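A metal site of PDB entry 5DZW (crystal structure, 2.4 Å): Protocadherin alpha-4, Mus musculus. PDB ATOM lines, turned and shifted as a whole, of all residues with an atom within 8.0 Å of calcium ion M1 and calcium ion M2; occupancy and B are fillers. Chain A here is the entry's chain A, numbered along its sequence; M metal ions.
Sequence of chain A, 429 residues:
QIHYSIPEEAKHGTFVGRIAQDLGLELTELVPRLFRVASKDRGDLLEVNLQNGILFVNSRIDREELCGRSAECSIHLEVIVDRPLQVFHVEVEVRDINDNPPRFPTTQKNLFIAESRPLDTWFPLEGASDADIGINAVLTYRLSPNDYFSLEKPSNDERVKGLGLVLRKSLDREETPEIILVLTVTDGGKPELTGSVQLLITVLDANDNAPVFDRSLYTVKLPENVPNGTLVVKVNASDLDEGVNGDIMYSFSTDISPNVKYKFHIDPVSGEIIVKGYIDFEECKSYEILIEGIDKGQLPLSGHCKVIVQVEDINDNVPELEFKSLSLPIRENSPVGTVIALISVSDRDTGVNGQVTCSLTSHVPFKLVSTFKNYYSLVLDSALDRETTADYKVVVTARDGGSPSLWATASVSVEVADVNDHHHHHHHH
Calcium ion M2 is bound by OE2 of Glu 64, OE1 of Glu 64, OD2 of Asp 99, OE1 of Glu 8 and OD1 of Asp 99.
Slightly farther from calcium ion M2 lies the side-chain carboxylate (OE2) of Glu 9 (3.1 Å).
Slightly farther from calcium ion M2 lies the side-chain carboxylate (OE2) of Glu 8 (3.1 Å).
Merely in contact with calcium ion M1: Asp 132 (3.2 Å).
Within 4 Å of calcium ion M1: Glu 8, Glu 64, Asp 96, Ile 97, Asp 99 and Asp 132.
The nearest printed residue that does not touch calcium ion M1 is Arg 63 (4.4 Å).
Calcium ion M1 is bound by OD2 of Asp 96, 2.4 Å away.
OE2 of Glu 8 is bound to calcium ion M1 (2.4 Å).
OE2 of Glu 64 binds calcium ion M1 (2.4 Å).
Calcium ion M1 is bound by O of Ile 97, at 2.6 Å.
Slightly farther from calcium ion M1 lies OD1 of Asp 99 (3.0 Å).
NH2 of Arg 63 sits close to OD2 of Asp 96.
N of Glu 8 sits at hydrogen-bond distance from O of Arg 95 (3.1 Å).
The side-chain carboxylate (OE2) of Glu 64 sits close to the side-chain amide nitrogen (ND2) of Asn 100, at 3.1 Å.
N of Asp 99 lies within hydrogen-bond range of OD2 of Asp 132, at 3.4 Å.
The side-chain carboxylate (OE1) of Glu 9 lies within salt-bridge range of the guanidinium group (NE) of Arg 60, at 2.7 Å.
The backbone carbonyl oxygen (O) of Ile 61 sits at hydrogen-bond distance from the backbone NH (N) of Glu 9, 2.8 Å away.
OD1 of Asp 132 lies close to ND2 of Asn 100, at 3.4 Å.
The side-chain amide oxygen (OD1) of Asn 98 lies close to the side-chain carboxylate (OD2) of Asp 132, at 3.2 Å.
Asp 62 touches calcium ion M2 (OD1 to CA, 3.2 Å).
Within 4 Å of calcium ion M2: Glu 8, Glu 9, Asp 62, Glu 64 and Asp 99.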
ATOM      1  N   GLU A   8      18.501 -16.043   5.916  1.00  0.00           N
ATOM      2  CA  GLU A   8      19.406 -16.932   5.195  1.00  0.00           C
ATOM      3  C   GLU A   8      20.818 -16.364   5.077  1.00  0.00           C
ATOM      4  O   GLU A   8      21.061 -15.211   5.455  1.00  0.00           O
ATOM      5  CB  GLU A   8      18.863 -17.227   3.801  1.00  0.00           C
ATOM      6  CG  GLU A   8      18.606 -15.967   2.978  1.00  0.00           C
ATOM      7  CD  GLU A   8      18.620 -16.236   1.494  1.00  0.00           C
ATOM      8  OE1 GLU A   8      19.221 -17.250   1.081  1.00  0.00           O
ATOM      9  OE2 GLU A   8      18.041 -15.431   0.737  1.00  0.00           O
ATOM     10  N   GLU A   9      21.736 -17.178   4.563  1.00  0.00           N
ATOM     11  CA  GLU A   9      23.113 -16.765   4.282  1.00  0.00           C
ATOM     12  C   GLU A   9      23.794 -16.153   5.509  1.00  0.00           C
ATOM     13  O   GLU A   9      24.611 -15.243   5.383  1.00  0.00           O
ATOM     14  CB  GLU A   9      23.137 -15.767   3.129  1.00  0.00           C
ATOM     15  CG  GLU A   9      22.410 -16.231   1.872  1.00  0.00           C
ATOM     16  CD  GLU A   9      23.200 -17.245   1.060  1.00  0.00           C
ATOM     17  OE1 GLU A   9      24.330 -17.586   1.462  1.00  0.00           O
ATOM     18  OE2 GLU A   9      22.684 -17.703   0.024  1.00  0.00           O
ATOM     19  N   ARG A  60      26.586 -22.925   5.522  1.00  0.00           N
ATOM     20  CA  ARG A  60      25.890 -21.918   4.729  1.00  0.00           C
ATOM     21  C   ARG A  60      24.462 -22.331   4.427  1.00  0.00           C
ATOM     22  O   ARG A  60      24.222 -23.386   3.839  1.00  0.00           O
ATOM     23  CB  ARG A  60      26.640 -21.635   3.428  1.00  0.00           C
ATOM     24  CG  ARG A  60      25.936 -20.642   2.510  1.00  0.00           C
ATOM     25  CD  ARG A  60      26.794 -20.295   1.297  1.00  0.00           C
ATOM     26  NE  ARG A  60      26.156 -19.314   0.433  1.00  0.00           N
ATOM     27  CZ  ARG A  60      25.474 -19.616  -0.669  1.00  0.00           C
ATOM     28  NH1 ARG A  60      25.336 -20.879  -1.050  1.00  0.00           N
ATOM     29  NH2 ARG A  60      24.921 -18.657  -1.391  1.00  0.00           N
ATOM     30  N   ILE A  61      23.507 -21.496   4.824  1.00  0.00           N
ATOM     31  CA  ILE A  61      22.101 -21.761   4.586  1.00  0.00           C
ATOM     32  C   ILE A  61      21.573 -20.929   3.418  1.00  0.00           C
ATOM     33  O   ILE A  61      21.177 -19.777   3.595  1.00  0.00           O
ATOM     34  CB  ILE A  61      21.253 -21.478   5.847  1.00  0.00           C
ATOM     35  CG1 ILE A  61      21.834 -22.200   7.060  1.00  0.00           C
ATOM     36  CG2 ILE A  61      19.801 -21.881   5.619  1.00  0.00           C
ATOM     37  CD1 ILE A  61      21.075 -21.963   8.343  1.00  0.00           C
ATOM     38  N   ASP A  62      21.594 -21.523   2.230  1.00  0.00           N
ATOM     39  CA  ASP A  62      21.104 -20.851   1.027  1.00  0.00           C
ATOM     40  C   ASP A  62      19.621 -21.170   0.824  1.00  0.00           C
ATOM     41  O   ASP A  62      19.265 -22.303   0.476  1.00  0.00           O
ATOM     42  CB  ASP A  62      21.915 -21.285  -0.197  1.00  0.00           C
ATOM     43  CG  ASP A  62      21.767 -20.337  -1.374  1.00  0.00           C
ATOM     44  OD1 ASP A  62      20.708 -19.693  -1.502  1.00  0.00           O
ATOM     45  OD2 ASP A  62      22.715 -20.247  -2.178  1.00  0.00           O
ATOM     46  N   ARG A  63      18.775 -20.179   1.050  1.00  0.00           N
ATOM     47  CA  ARG A  63      17.329 -20.378   1.048  1.00  0.00           C
ATOM     48  C   ARG A  63      16.802 -20.906  -0.286  1.00  0.00           C
ATOM     49  O   ARG A  63      15.994 -21.848  -0.307  1.00  0.00           O
ATOM     50  CB  ARG A  63      16.616 -19.072   1.396  1.00  0.00           C
ATOM     51  CG  ARG A  63      15.114 -19.173   1.298  1.00  0.00           C
ATOM     52  CD  ARG A  63      14.462 -17.805   1.384  1.00  0.00           C
ATOM     53  NE  ARG A  63      13.107 -17.838   0.856  1.00  0.00           N
ATOM     54  CZ  ARG A  63      12.809 -17.739  -0.435  1.00  0.00           C
ATOM     55  NH1 ARG A  63      11.550 -17.782  -0.837  1.00  0.00           N
ATOM     56  NH2 ARG A  63      13.782 -17.598  -1.335  1.00  0.00           N
ATOM     57  N   GLU A  64      17.249 -20.307  -1.379  1.00  0.00           N
ATOM     58  CA  GLU A  64      16.759 -20.658  -2.711  1.00  0.00           C
ATOM     59  C   GLU A  64      17.151 -22.074  -3.114  1.00  0.00           C
ATOM     60  O   GLU A  64      16.557 -22.656  -4.017  1.00  0.00           O
ATOM     61  CB  GLU A  64      17.292 -19.660  -3.749  1.00  0.00           C
ATOM     62  CG  GLU A  64      16.924 -18.204  -3.484  1.00  0.00           C
ATOM     63  CD  GLU A  64      17.896 -17.512  -2.558  1.00  0.00           C
ATOM     64  OE1 GLU A  64      18.234 -18.085  -1.500  1.00  0.00           O
ATOM     65  OE2 GLU A  64      18.332 -16.392  -2.889  1.00  0.00           O
ATOM     66  N   GLU A  65      18.158 -22.634  -2.439  1.00  0.00           N
ATOM     67  CA  GLU A  65      18.590 -23.993  -2.714  1.00  0.00           C
ATOM     68  C   GLU A  65      17.764 -24.985  -1.916  1.00  0.00           C
ATOM     69  O   GLU A  65      17.790 -26.193  -2.165  1.00  0.00           O
ATOM     70  CB  GLU A  65      20.080 -24.148  -2.408  1.00  0.00           C
ATOM     71  CG  GLU A  65      20.720 -25.391  -3.025  1.00  0.00           C
ATOM     72  CD  GLU A  65      22.228 -25.387  -2.902  1.00  0.00           C
ATOM     73  OE1 GLU A  65      22.792 -24.398  -2.387  1.00  0.00           O
ATOM     74  OE2 GLU A  65      22.870 -26.373  -3.344  1.00  0.00           O
ATOM     75  N   GLY A  68      13.439 -22.994  -2.635  1.00  0.00           N
ATOM     76  CA  GLY A  68      13.413 -22.576  -4.028  1.00  0.00           C
ATOM     77  C   GLY A  68      12.490 -21.399  -4.265  1.00  0.00           C
ATOM     78  O   GLY A  68      12.690 -20.323  -3.713  1.00  0.00           O
ATOM     79  N   ARG A  95      14.091 -16.700   6.615  1.00  0.00           N
ATOM     80  CA  ARG A  95      13.611 -15.512   5.927  1.00  0.00           C
ATOM     81  C   ARG A  95      14.473 -15.186   4.713  1.00  0.00           C
ATOM     82  O   ARG A  95      15.678 -15.427   4.713  1.00  0.00           O
ATOM     83  CB  ARG A  95      13.547 -14.320   6.885  1.00  0.00           C
ATOM     84  CG  ARG A  95      12.577 -14.519   8.030  1.00  0.00           C
ATOM     85  CD  ARG A  95      12.576 -13.338   8.996  1.00  0.00           C
ATOM     86  NE  ARG A  95      13.862 -13.169   9.648  1.00  0.00           N
ATOM     87  CZ  ARG A  95      14.069 -12.364  10.691  1.00  0.00           C
ATOM     88  NH1 ARG A  95      13.062 -11.674  11.210  1.00  0.00           N
ATOM     89  NH2 ARG A  95      15.276 -12.271  11.226  1.00  0.00           N
ATOM     90  N   ASP A  96      13.832 -14.628   3.692  1.00  0.00           N
ATOM     91  CA  ASP A  96      14.501 -14.331   2.429  1.00  0.00           C
ATOM     92  C   ASP A  96      15.384 -13.093   2.512  1.00  0.00           C
ATOM     93  O   ASP A  96      15.023 -12.092   3.113  1.00  0.00           O
ATOM     94  CB  ASP A  96      13.467 -14.158   1.316  1.00  0.00           C
ATOM     95  CG  ASP A  96      14.088 -13.903  -0.043  1.00  0.00           C
ATOM     96  OD1 ASP A  96      13.592 -13.018  -0.772  1.00  0.00           O
ATOM     97  OD2 ASP A  96      15.085 -14.582  -0.381  1.00  0.00           O
ATOM     98  N   ILE A  97      16.565 -13.188   1.899  1.00  0.00           N
ATOM     99  CA  ILE A  97      17.470 -12.049   1.773  1.00  0.00           C
ATOM    100  C   ILE A  97      17.688 -11.708   0.309  1.00  0.00           C
ATOM    101  O   ILE A  97      17.996 -12.590  -0.502  1.00  0.00           O
ATOM    102  CB  ILE A  97      18.823 -12.330   2.453  1.00  0.00           C
ATOM    103  CG1 ILE A  97      18.678 -12.310   3.970  1.00  0.00           C
ATOM    104  CG2 ILE A  97      19.875 -11.313   2.016  1.00  0.00           C
ATOM    105  CD1 ILE A  97      19.996 -12.318   4.717  1.00  0.00           C
ATOM    106  N   ASN A  98      17.527 -10.434  -0.036  1.00  0.00           N
ATOM    107  CA  ASN A  98      17.700  -9.989  -1.416  1.00  0.00           C
ATOM    108  C   ASN A  98      19.162 -10.034  -1.849  1.00  0.00           C
ATOM    109  O   ASN A  98      19.811  -9.003  -1.980  1.00  0.00           O
ATOM    110  CB  ASN A  98      17.152  -8.566  -1.597  1.00  0.00           C
ATOM    111  CG  ASN A  98      16.967  -8.183  -3.052  1.00  0.00           C
ATOM    112  OD1 ASN A  98      16.972  -9.043  -3.933  1.00  0.00           O
ATOM    113  ND2 ASN A  98      16.799  -6.892  -3.307  1.00  0.00           N
ATOM    114  N   ASP A  99      19.677 -11.242  -2.054  1.00  0.00           N
ATOM    115  CA  ASP A  99      21.082 -11.418  -2.415  1.00  0.00           C
ATOM    116  C   ASP A  99      21.253 -11.894  -3.852  1.00  0.00           C
ATOM    117  O   ASP A  99      22.347 -12.269  -4.274  1.00  0.00           O
ATOM    118  CB  ASP A  99      21.775 -12.392  -1.452  1.00  0.00           C
ATOM    119  CG  ASP A  99      21.178 -13.792  -1.502  1.00  0.00           C
ATOM    120  OD1 ASP A  99      19.994 -13.931  -1.865  1.00  0.00           O
ATOM    121  OD2 ASP A  99      21.908 -14.758  -1.172  1.00  0.00           O
ATOM    122  N   ASN A 100      20.155 -11.885  -4.613  1.00  0.00           N
ATOM    123  CA  ASN A 100      20.202 -12.214  -6.038  1.00  0.00           C
ATOM    124  C   ASN A 100      19.563 -11.128  -6.898  1.00  0.00           C
ATOM    125  O   ASN A 100      18.436 -10.715  -6.641  1.00  0.00           O
ATOM    126  CB  ASN A 100      19.523 -13.556  -6.290  1.00  0.00           C
ATOM    127  CG  ASN A 100      20.349 -14.733  -5.836  1.00  0.00           C
ATOM    128  OD1 ASN A 100      21.566 -14.635  -5.694  1.00  0.00           O
ATOM    129  ND2 ASN A 100      19.692 -15.862  -5.601  1.00  0.00           N
ATOM    130  N   ASP A 130      13.858 -13.883 -11.388  1.00  0.00           N
ATOM    131  CA  ASP A 130      14.518 -13.668 -10.106  1.00  0.00           C
ATOM    132  C   ASP A 130      14.400 -14.905  -9.227  1.00  0.00           C
ATOM    133  O   ASP A 130      13.336 -15.526  -9.149  1.00  0.00           O
ATOM    134  CB  ASP A 130      13.941 -12.448  -9.397  1.00  0.00           C
ATOM    135  CG  ASP A 130      14.837 -11.927  -8.296  1.00  0.00           C
ATOM    136  OD1 ASP A 130      16.072 -11.895  -8.505  1.00  0.00           O
ATOM    137  OD2 ASP A 130      14.313 -11.571  -7.223  1.00  0.00           O
ATOM    138  N   ALA A 131      15.495 -15.271  -8.573  1.00  0.00           N
ATOM    139  CA  ALA A 131      15.526 -16.456  -7.727  1.00  0.00           C
ATOM    140  C   ALA A 131      14.821 -16.219  -6.395  1.00  0.00           C
ATOM    141  O   ALA A 131      14.270 -17.135  -5.796  1.00  0.00           O
ATOM    142  CB  ALA A 131      16.964 -16.907  -7.493  1.00  0.00           C
ATOM    143  N   ASP A 132      14.845 -14.961  -5.940  1.00  0.00           N
ATOM    144  CA  ASP A 132      14.247 -14.598  -4.668  1.00  0.00           C
ATOM    145  C   ASP A 132      12.721 -14.594  -4.752  1.00  0.00           C
ATOM    146  O   ASP A 132      12.152 -14.645  -5.839  1.00  0.00           O
ATOM    147  CB  ASP A 132      14.756 -13.228  -4.221  1.00  0.00           C
ATOM    148  CG  ASP A 132      16.260 -13.195  -4.047  1.00  0.00           C
ATOM    149  OD1 ASP A 132      16.930 -14.152  -4.504  1.00  0.00           O
ATOM    150  OD2 ASP A 132      16.776 -12.219  -3.472  1.00  0.00           O
ATOM    151  N   ILE A 133      12.070 -14.539  -3.594  1.00  0.00           N
ATOM    152  CA  ILE A 133      10.616 -14.555  -3.524  1.00  0.00           C
ATOM    153  C   ILE A 133      10.102 -13.476  -2.581  1.00  0.00           C
ATOM    154  O   ILE A 133      10.616 -13.324  -1.470  1.00  0.00           O
ATOM    155  CB  ILE A 133      10.078 -15.932  -3.070  1.00  0.00           C
ATOM    156  CG1 ILE A 133      10.482 -17.036  -4.067  1.00  0.00           C
ATOM    157  CG2 ILE A 133       8.562 -15.901  -2.927  1.00  0.00           C
ATOM    158  CD1 ILE A 133       9.864 -16.876  -5.439  1.00  0.00           C
ATOM    159  N   ASN A 136      11.497  -8.862  -2.607  1.00  0.00           N
ATOM    160  CA  ASN A 136      12.803  -8.984  -3.254  1.00  0.00           C
ATOM    161  C   ASN A 136      12.677  -9.464  -4.694  1.00  0.00           C
ATOM    162  O   ASN A 136      13.632  -9.393  -5.462  1.00  0.00           O
ATOM    163  CB  ASN A 136      13.704  -9.929  -2.463  1.00  0.00           C
ATOM    164  CG  ASN A 136      13.853  -9.524  -1.007  1.00  0.00           C
ATOM    165  OD1 ASN A 136      13.685  -8.355  -0.660  1.00  0.00           O
ATOM    166  ND2 ASN A 136      14.169 -10.490  -0.148  1.00  0.00           N
HETATM  167 CA    CA M   1      17.183 -14.842  -1.415  1.00  0.00          CA
HETATM  168 CA    CA M   2      20.136 -16.533  -1.213  1.00  0.00          CA
HETATM  169 CA    CA M   3      16.096 -10.501  -5.773  1.00  0.00          CA
